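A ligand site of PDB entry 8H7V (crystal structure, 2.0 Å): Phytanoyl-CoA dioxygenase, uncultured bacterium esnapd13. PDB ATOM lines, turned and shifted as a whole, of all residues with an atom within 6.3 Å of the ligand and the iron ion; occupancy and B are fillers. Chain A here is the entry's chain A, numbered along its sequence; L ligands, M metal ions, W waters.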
ATOM      1  N   HIS A  65      -0.971  -1.007  -7.225  1.00  0.00           N
ATOM      2  CA  HIS A  65      -2.170  -0.489  -7.872  1.00  0.00           C
ATOM      3  C   HIS A  65      -3.438  -0.992  -7.189  1.00  0.00           C
ATOM      4  O   HIS A  65      -3.480  -2.139  -6.741  1.00  0.00           O
ATOM      5  CB  HIS A  65      -2.192  -0.885  -9.352  1.00  0.00           C
ATOM      6  CG  HIS A  65      -1.216  -0.160 -10.231  1.00  0.00           C
ATOM      7  ND1 HIS A  65       0.125  -0.453 -10.283  1.00  0.00           N
ATOM      8  CD2 HIS A  65      -1.447   0.844 -11.116  1.00  0.00           C
ATOM      9  CE1 HIS A  65       0.705   0.354 -11.166  1.00  0.00           C
ATOM     10  NE2 HIS A  65      -0.250   1.166 -11.692  1.00  0.00           N
ATOM     11  N   GLN A  99      -8.415   4.958 -11.249  1.00  0.00           N
ATOM     12  CA  GLN A  99      -7.162   4.292 -10.966  1.00  0.00           C
ATOM     13  C   GLN A  99      -6.581   4.834  -9.654  1.00  0.00           C
ATOM     14  O   GLN A  99      -6.755   6.012  -9.329  1.00  0.00           O
ATOM     15  CB  GLN A  99      -6.194   4.536 -12.121  1.00  0.00           C
ATOM     16  CG  GLN A  99      -4.923   3.702 -12.033  1.00  0.00           C
ATOM     17  CD  GLN A  99      -4.074   3.894 -13.268  1.00  0.00           C
ATOM     18  OE1 GLN A  99      -4.045   3.037 -14.151  1.00  0.00           O
ATOM     19  NE2 GLN A  99      -3.401   5.028 -13.334  1.00  0.00           N
ATOM     20  N   LYS A 101      -2.791   4.404  -7.482  1.00  0.00           N
ATOM     21  CA  LYS A 101      -1.459   3.830  -7.403  1.00  0.00           C
ATOM     22  C   LYS A 101      -0.625   4.555  -6.357  1.00  0.00           C
ATOM     23  O   LYS A 101      -0.833   5.730  -6.069  1.00  0.00           O
ATOM     24  CB  LYS A 101      -0.781   3.826  -8.778  1.00  0.00           C
ATOM     25  CG  LYS A 101      -0.558   5.189  -9.416  1.00  0.00           C
ATOM     26  CD  LYS A 101       0.329   5.157 -10.639  1.00  0.00           C
ATOM     27  CE  LYS A 101      -0.350   4.605 -11.873  1.00  0.00           C
ATOM     28  NZ  LYS A 101       0.589   4.498 -13.021  1.00  0.00           N
ATOM     29  N   ASN A 103       3.415   5.233  -5.803  1.00  0.00           N
ATOM     30  CA  ASN A 103       4.741   5.205  -6.410  1.00  0.00           C
ATOM     31  C   ASN A 103       5.758   5.690  -5.393  1.00  0.00           C
ATOM     32  O   ASN A 103       5.745   6.866  -5.004  1.00  0.00           O
ATOM     33  CB  ASN A 103       4.843   6.084  -7.660  1.00  0.00           C
ATOM     34  CG  ASN A 103       4.072   5.549  -8.844  1.00  0.00           C
ATOM     35  OD1 ASN A 103       3.500   4.466  -8.799  1.00  0.00           O
ATOM     36  ND2 ASN A 103       4.075   6.313  -9.929  1.00  0.00           N
ATOM     37  N   ALA A 104       6.619   4.771  -4.950  1.00  0.00           N
ATOM     38  CA  ALA A 104       7.719   5.085  -4.054  1.00  0.00           C
ATOM     39  C   ALA A 104       8.971   5.310  -4.897  1.00  0.00           C
ATOM     40  O   ALA A 104       9.299   4.495  -5.754  1.00  0.00           O
ATOM     41  CB  ALA A 104       7.929   3.966  -3.067  1.00  0.00           C
ATOM     42  N   LYS A 105       9.636   6.438  -4.672  1.00  0.00           N
ATOM     43  CA  LYS A 105      10.986   6.656  -5.156  1.00  0.00           C
ATOM     44  C   LYS A 105      11.910   6.762  -3.956  1.00  0.00           C
ATOM     45  O   LYS A 105      11.982   7.825  -3.329  1.00  0.00           O
ATOM     46  CB  LYS A 105      11.074   7.928  -5.997  1.00  0.00           C
ATOM     47  CG  LYS A 105      10.822   7.742  -7.479  1.00  0.00           C
ATOM     48  CD  LYS A 105      11.235   8.963  -8.253  1.00  0.00           C
ATOM     49  CE  LYS A 105      10.680   8.925  -9.648  1.00  0.00           C
ATOM     50  NZ  LYS A 105      10.808  10.237 -10.308  1.00  0.00           N
ATOM     51  N   GLU A 111      13.693   5.739 -11.023  1.00  0.00           N
ATOM     52  CA  GLU A 111      13.943   5.611 -12.447  1.00  0.00           C
ATOM     53  C   GLU A 111      13.412   6.857 -13.155  1.00  0.00           C
ATOM     54  O   GLU A 111      12.675   7.643 -12.568  1.00  0.00           O
ATOM     55  CB  GLU A 111      13.258   4.353 -12.999  1.00  0.00           C
ATOM     56  CG  GLU A 111      13.786   3.066 -12.397  1.00  0.00           C
ATOM     57  CD  GLU A 111      12.955   1.837 -12.723  1.00  0.00           C
ATOM     58  OE1 GLU A 111      12.831   1.506 -13.917  1.00  0.00           O
ATOM     59  OE2 GLU A 111      12.431   1.207 -11.766  1.00  0.00           O
ATOM     60  N   TRP A 113      10.867   8.397 -15.495  1.00  0.00           N
ATOM     61  CA  TRP A 113       9.583   8.275 -16.149  1.00  0.00           C
ATOM     62  C   TRP A 113       9.578   9.157 -17.390  1.00  0.00           C
ATOM     63  O   TRP A 113       9.615  10.391 -17.278  1.00  0.00           O
ATOM     64  CB  TRP A 113       8.426   8.647 -15.211  1.00  0.00           C
ATOM     65  CG  TRP A 113       8.116   7.582 -14.197  1.00  0.00           C
ATOM     66  CD1 TRP A 113       8.864   7.245 -13.107  1.00  0.00           C
ATOM     67  CD2 TRP A 113       6.976   6.716 -14.192  1.00  0.00           C
ATOM     68  NE1 TRP A 113       8.252   6.227 -12.412  1.00  0.00           N
ATOM     69  CE2 TRP A 113       7.087   5.890 -13.053  1.00  0.00           C
ATOM     70  CE3 TRP A 113       5.857   6.566 -15.022  1.00  0.00           C
ATOM     71  CZ2 TRP A 113       6.142   4.923 -12.729  1.00  0.00           C
ATOM     72  CZ3 TRP A 113       4.916   5.608 -14.700  1.00  0.00           C
ATOM     73  CH2 TRP A 113       5.059   4.800 -13.571  1.00  0.00           C
ATOM     74  N   HIS A 116       4.889  11.576 -20.801  1.00  0.00           N
ATOM     75  CA  HIS A 116       3.635  10.949 -21.197  1.00  0.00           C
ATOM     76  C   HIS A 116       2.440  11.776 -20.738  1.00  0.00           C
ATOM     77  O   HIS A 116       2.583  12.655 -19.875  1.00  0.00           O
ATOM     78  CB  HIS A 116       3.543   9.525 -20.635  1.00  0.00           C
ATOM     79  CG  HIS A 116       3.470   9.468 -19.137  1.00  0.00           C
ATOM     80  ND1 HIS A 116       4.534   9.707 -18.313  1.00  0.00           N
ATOM     81  CD2 HIS A 116       2.392   9.203 -18.336  1.00  0.00           C
ATOM     82  CE1 HIS A 116       4.135   9.593 -17.040  1.00  0.00           C
ATOM     83  NE2 HIS A 116       2.801   9.287 -17.036  1.00  0.00           N
ATOM     84  N   GLN A 117       1.278  11.479 -21.337  1.00  0.00           N
ATOM     85  CA  GLN A 117      -0.011  11.953 -20.858  1.00  0.00           C
ATOM     86  C   GLN A 117      -0.800  10.736 -20.389  1.00  0.00           C
ATOM     87  O   GLN A 117      -0.958   9.767 -21.126  1.00  0.00           O
ATOM     88  CB  GLN A 117      -0.757  12.681 -21.980  1.00  0.00           C
ATOM     89  CG  GLN A 117      -0.061  13.943 -22.484  1.00  0.00           C
ATOM     90  CD  GLN A 117      -0.610  14.412 -23.819  1.00  0.00           C
ATOM     91  OE1 GLN A 117      -0.505  13.719 -24.826  1.00  0.00           O
ATOM     92  NE2 GLN A 117      -1.207  15.597 -23.837  1.00  0.00           N
ATOM     93  N   ASP A 118      -1.305  10.784 -19.147  1.00  0.00           N
ATOM     94  CA  ASP A 118      -2.056   9.667 -18.589  1.00  0.00           C
ATOM     95  C   ASP A 118      -3.258   9.331 -19.485  1.00  0.00           C
ATOM     96  O   ASP A 118      -3.600   8.163 -19.652  1.00  0.00           O
ATOM     97  CB  ASP A 118      -2.512   9.952 -17.156  1.00  0.00           C
ATOM     98  CG  ASP A 118      -1.385  10.099 -16.151  1.00  0.00           C
ATOM     99  OD1 ASP A 118      -0.267   9.576 -16.409  1.00  0.00           O
ATOM    100  OD2 ASP A 118      -1.613  10.762 -15.114  1.00  0.00           O
ATOM    101  N   GLY A 148      13.250  13.600  -7.336  1.00  0.00           N
ATOM    102  CA  GLY A 148      12.534  13.091  -8.494  1.00  0.00           C
ATOM    103  C   GLY A 148      11.092  13.570  -8.565  1.00  0.00           C
ATOM    104  O   GLY A 148      10.180  12.766  -8.758  1.00  0.00           O
ATOM    105  N   PRO A 149      10.838  14.892  -8.476  1.00  0.00           N
ATOM    106  CA  PRO A 149       9.480  15.425  -8.540  1.00  0.00           C
ATOM    107  C   PRO A 149       8.821  15.185  -9.897  1.00  0.00           C
ATOM    108  O   PRO A 149       9.502  15.179 -10.924  1.00  0.00           O
ATOM    109  CB  PRO A 149       9.681  16.938  -8.335  1.00  0.00           C
ATOM    110  CG  PRO A 149      11.088  17.192  -8.846  1.00  0.00           C
ATOM    111  CD  PRO A 149      11.859  15.955  -8.419  1.00  0.00           C
ATOM    112  N   LEU A 150       7.494  15.009  -9.891  1.00  0.00           N
ATOM    113  CA  LEU A 150       6.730  15.092 -11.125  1.00  0.00           C
ATOM    114  C   LEU A 150       7.006  16.454 -11.768  1.00  0.00           C
ATOM    115  O   LEU A 150       6.951  17.481 -11.096  1.00  0.00           O
ATOM    116  CB  LEU A 150       5.232  14.948 -10.822  1.00  0.00           C
ATOM    117  CG  LEU A 150       4.769  13.570 -10.342  1.00  0.00           C
ATOM    118  CD1 LEU A 150       3.278  13.585 -10.058  1.00  0.00           C
ATOM    119  CD2 LEU A 150       5.096  12.509 -11.380  1.00  0.00           C
ATOM    120  N   PHE A 210      -3.519  17.335 -10.839  1.00  0.00           N
ATOM    121  CA  PHE A 210      -3.093  17.537 -12.223  1.00  0.00           C
ATOM    122  C   PHE A 210      -4.027  16.837 -13.198  1.00  0.00           C
ATOM    123  O   PHE A 210      -4.606  15.790 -12.923  1.00  0.00           O
ATOM    124  CB  PHE A 210      -1.632  17.150 -12.438  1.00  0.00           C
ATOM    125  CG  PHE A 210      -1.261  15.707 -12.201  1.00  0.00           C
ATOM    126  CD1 PHE A 210      -0.953  15.253 -10.930  1.00  0.00           C
ATOM    127  CD2 PHE A 210      -1.172  14.813 -13.254  1.00  0.00           C
ATOM    128  CE1 PHE A 210      -0.591  13.930 -10.718  1.00  0.00           C
ATOM    129  CE2 PHE A 210      -0.799  13.495 -13.050  1.00  0.00           C
ATOM    130  CZ  PHE A 210      -0.511  13.050 -11.774  1.00  0.00           C
ATOM    131  N   HIS A 216       3.815  14.895 -18.393  1.00  0.00           N
ATOM    132  CA  HIS A 216       4.713  14.902 -17.253  1.00  0.00           C
ATOM    133  C   HIS A 216       5.752  13.797 -17.371  1.00  0.00           C
ATOM    134  O   HIS A 216       5.618  12.854 -18.148  1.00  0.00           O
ATOM    135  CB  HIS A 216       3.941  14.792 -15.938  1.00  0.00           C
ATOM    136  CG  HIS A 216       2.993  13.646 -15.859  1.00  0.00           C
ATOM    137  ND1 HIS A 216       1.798  13.606 -16.520  1.00  0.00           N
ATOM    138  CD2 HIS A 216       3.091  12.489 -15.150  1.00  0.00           C
ATOM    139  CE1 HIS A 216       1.170  12.462 -16.233  1.00  0.00           C
ATOM    140  NE2 HIS A 216       1.951  11.752 -15.395  1.00  0.00           N
ATOM    141  N   SER A 217       6.803  13.962 -16.561  1.00  0.00           N
ATOM    142  CA  SER A 217       7.978  13.104 -16.530  1.00  0.00           C
ATOM    143  C   SER A 217       8.615  13.258 -15.156  1.00  0.00           C
ATOM    144  O   SER A 217       8.215  14.132 -14.386  1.00  0.00           O
ATOM    145  CB  SER A 217       8.926  13.494 -17.658  1.00  0.00           C
ATOM    146  OG  SER A 217      10.181  12.841 -17.594  1.00  0.00           O
ATOM    147  N   SER A 218       9.549  12.375 -14.818  1.00  0.00           N
ATOM    148  CA  SER A 218      10.310  12.525 -13.583  1.00  0.00           C
ATOM    149  C   SER A 218      11.628  11.770 -13.676  1.00  0.00           C
ATOM    150  O   SER A 218      11.774  10.890 -14.527  1.00  0.00           O
ATOM    151  CB  SER A 218       9.513  12.096 -12.375  1.00  0.00           C
ATOM    152  OG  SER A 218       9.250  10.707 -12.420  1.00  0.00           O
ATOM    153  N   VAL A 219      12.562  12.140 -12.805  1.00  0.00           N
ATOM    154  CA  VAL A 219      13.927  11.632 -12.832  1.00  0.00           C
ATOM    155  C   VAL A 219      14.197  10.866 -11.541  1.00  0.00           C
ATOM    156  O   VAL A 219      13.379  10.877 -10.621  1.00  0.00           O
ATOM    157  CB  VAL A 219      14.939  12.777 -13.053  1.00  0.00           C
ATOM    158  CG1 VAL A 219      14.589  13.615 -14.269  1.00  0.00           C
ATOM    159  CG2 VAL A 219      15.097  13.655 -11.814  1.00  0.00           C
ATOM    160  N   ARG A 227      10.605   9.697  -1.759  1.00  0.00           N
ATOM    161  CA  ARG A 227       9.540  10.497  -2.366  1.00  0.00           C
ATOM    162  C   ARG A 227       8.341   9.594  -2.630  1.00  0.00           C
ATOM    163  O   ARG A 227       8.157   9.136  -3.756  1.00  0.00           O
ATOM    164  CB  ARG A 227      10.015  11.150  -3.655  1.00  0.00           C
ATOM    165  CG  ARG A 227       9.041  12.181  -4.235  1.00  0.00           C
ATOM    166  CD  ARG A 227       8.817  12.003  -5.725  1.00  0.00           C
ATOM    167  NE  ARG A 227       8.178  10.732  -6.005  1.00  0.00           N
ATOM    168  CZ  ARG A 227       7.738  10.330  -7.189  1.00  0.00           C
ATOM    169  NH1 ARG A 227       7.848  11.121  -8.240  1.00  0.00           N
ATOM    170  NH2 ARG A 227       7.163   9.151  -7.312  1.00  0.00           N
ATOM    171  N   LEU A 229       4.464   8.954  -3.308  1.00  0.00           N
ATOM    172  CA  LEU A 229       3.247   9.610  -3.791  1.00  0.00           C
ATOM    173  C   LEU A 229       2.096   8.605  -3.785  1.00  0.00           C
ATOM    174  O   LEU A 229       2.257   7.481  -4.260  1.00  0.00           O
ATOM    175  CB  LEU A 229       3.456  10.131  -5.222  1.00  0.00           C
ATOM    176  CG  LEU A 229       4.517  11.216  -5.414  1.00  0.00           C
ATOM    177  CD1 LEU A 229       4.594  11.633  -6.872  1.00  0.00           C
ATOM    178  CD2 LEU A 229       4.246  12.423  -4.527  1.00  0.00           C
ATOM    179  N   LEU A 231      -1.314   8.364  -5.657  1.00  0.00           N
ATOM    180  CA  LEU A 231      -1.950   8.995  -6.804  1.00  0.00           C
ATOM    181  C   LEU A 231      -3.340   8.431  -7.002  1.00  0.00           C
ATOM    182  O   LEU A 231      -3.499   7.259  -7.356  1.00  0.00           O
ATOM    183  CB  LEU A 231      -1.081   8.799  -8.052  1.00  0.00           C
ATOM    184  CG  LEU A 231       0.311   9.437  -7.985  1.00  0.00           C
ATOM    185  CD1 LEU A 231       1.385   8.368  -7.957  1.00  0.00           C
ATOM    186  CD2 LEU A 231       0.535  10.405  -9.126  1.00  0.00           C
HETATM  187  C1  LIG L   1       2.366   7.700 -13.598  1.00  0.00           C
HETATM  188  O1  LIG L   1       2.319   6.667 -12.921  1.00  0.00           O
HETATM  189  O2  LIG L   1       1.648   7.876 -14.596  1.00  0.00           O
HETATM  190  C2  LIG L   1       3.200   8.649 -13.229  1.00  0.00           C
HETATM  191  O3  LIG L   1       3.261   9.647 -13.948  1.00  0.00           O
HETATM  192  C3  LIG L   1       4.043   8.613 -11.973  1.00  0.00           C
HETATM  193  C4  LIG L   1       5.441   9.188 -12.103  1.00  0.00           C
HETATM  194  C5  LIG L   1       6.242   9.267 -10.807  1.00  0.00           C
HETATM  195  O4  LIG L   1       5.829   8.644  -9.797  1.00  0.00           O
HETATM  196  O5  LIG L   1       7.285   9.955 -10.802  1.00  0.00           O
HETATM  197 FE    FE M   1       1.618   9.771 -15.283  1.00  0.00          FE
HETATM  198  O   HOH W   1       0.382  10.070 -13.349  1.00  0.00           O
HETATM  199  O   HOH W   2      -1.153   6.464 -14.789  1.00  0.00           O
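Trp 113 touches the ligand (CZ3 to O1, 3.3 Å).
CD2 of Leu 150 touches O5 of the ligand, at 3.4 Å.
Hydrophobic or aromatic side chains that line the ligand: Trp 113, His 116, Leu 150 and His 216.
Ten residues have an atom within 4 Å of the ligand: Lys 101, Asn 103, Lys 105, Trp 113, His 116, Asp 118, Leu 150, His 216, Ser 218 and Arg 227.
The nearest printed residue that does not touch the ligand is Leu 229 (4.4 Å).
Three residues have an atom within 4 Å of the iron ion: His 116, Asp 118 and His 216.
The side-chain hydroxyl (OG) of Ser 218 is in hydrogen-bond range of the side-chain amino group (NZ) of Lys 105 (2.7 Å).
The backbone carbonyl oxygen (O) of Leu 229 sits at hydrogen-bond distance from the backbone NH (N) of Asn 103.
The backbone NH (N) of Trp 113 is in hydrogen-bond range of the backbone carbonyl oxygen (O) of Ser 218 (2.8 Å).
The backbone carbonyl oxygen (O) of Lys 101 sits at hydrogen-bond distance from the backbone NH (N) of Leu 231, 2.7 Å away.
O of Lys 105 lies within hydrogen-bond range of N of Arg 227 (2.8 Å).
O of Trp 113 sits at hydrogen-bond distance from OG of Ser 217 (2.5 Å).
NH1 of Arg 227 lies within hydrogen-bond range of O of Gly 148 (2.9 Å).
O of Gly 148 sits at hydrogen-bond distance from NZ of Lys 105 (3.0 Å).
The iron ion is bound by a ring nitrogen (NE2) of His 216 (2.0 Å), an oxygen (O2) of the ligand (2.0 Å), an oxygen (O3) of the ligand (2.1 Å), a ring nitrogen (NE2) of His 116 (2.2 Å), the side-chain carboxylate (OD1) of Asp 118 (2.2 Å) and water W1 (2.3 Å).
Water W2 lies within hydrogen-bond range of the side-chain amide nitrogen (NE2) of Gln 99 and the side-chain amino group (NZ) of Lys 101.
The side-chain amino group of Lys 101 is in salt-bridge range of an oxygen (O1) of the ligand (2.8 Å).
The side-chain amide nitrogen (ND2) of Asn 103 is in hydrogen-bond range of an oxygen (O4) of the ligand, 2.9 Å away.
The guanidinium group (NH2) of Arg 227 lies within salt-bridge range of an oxygen (O4) of the ligand, at 2.9 Å.
The side-chain hydroxyl of Ser 218 sits at hydrogen-bond distance from an oxygen (O5) of the ligand (2.7 Å).
The side-chain amino group of Lys 105 is in salt-bridge range of an oxygen (O5) of the ligand, at 3.6 Å.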
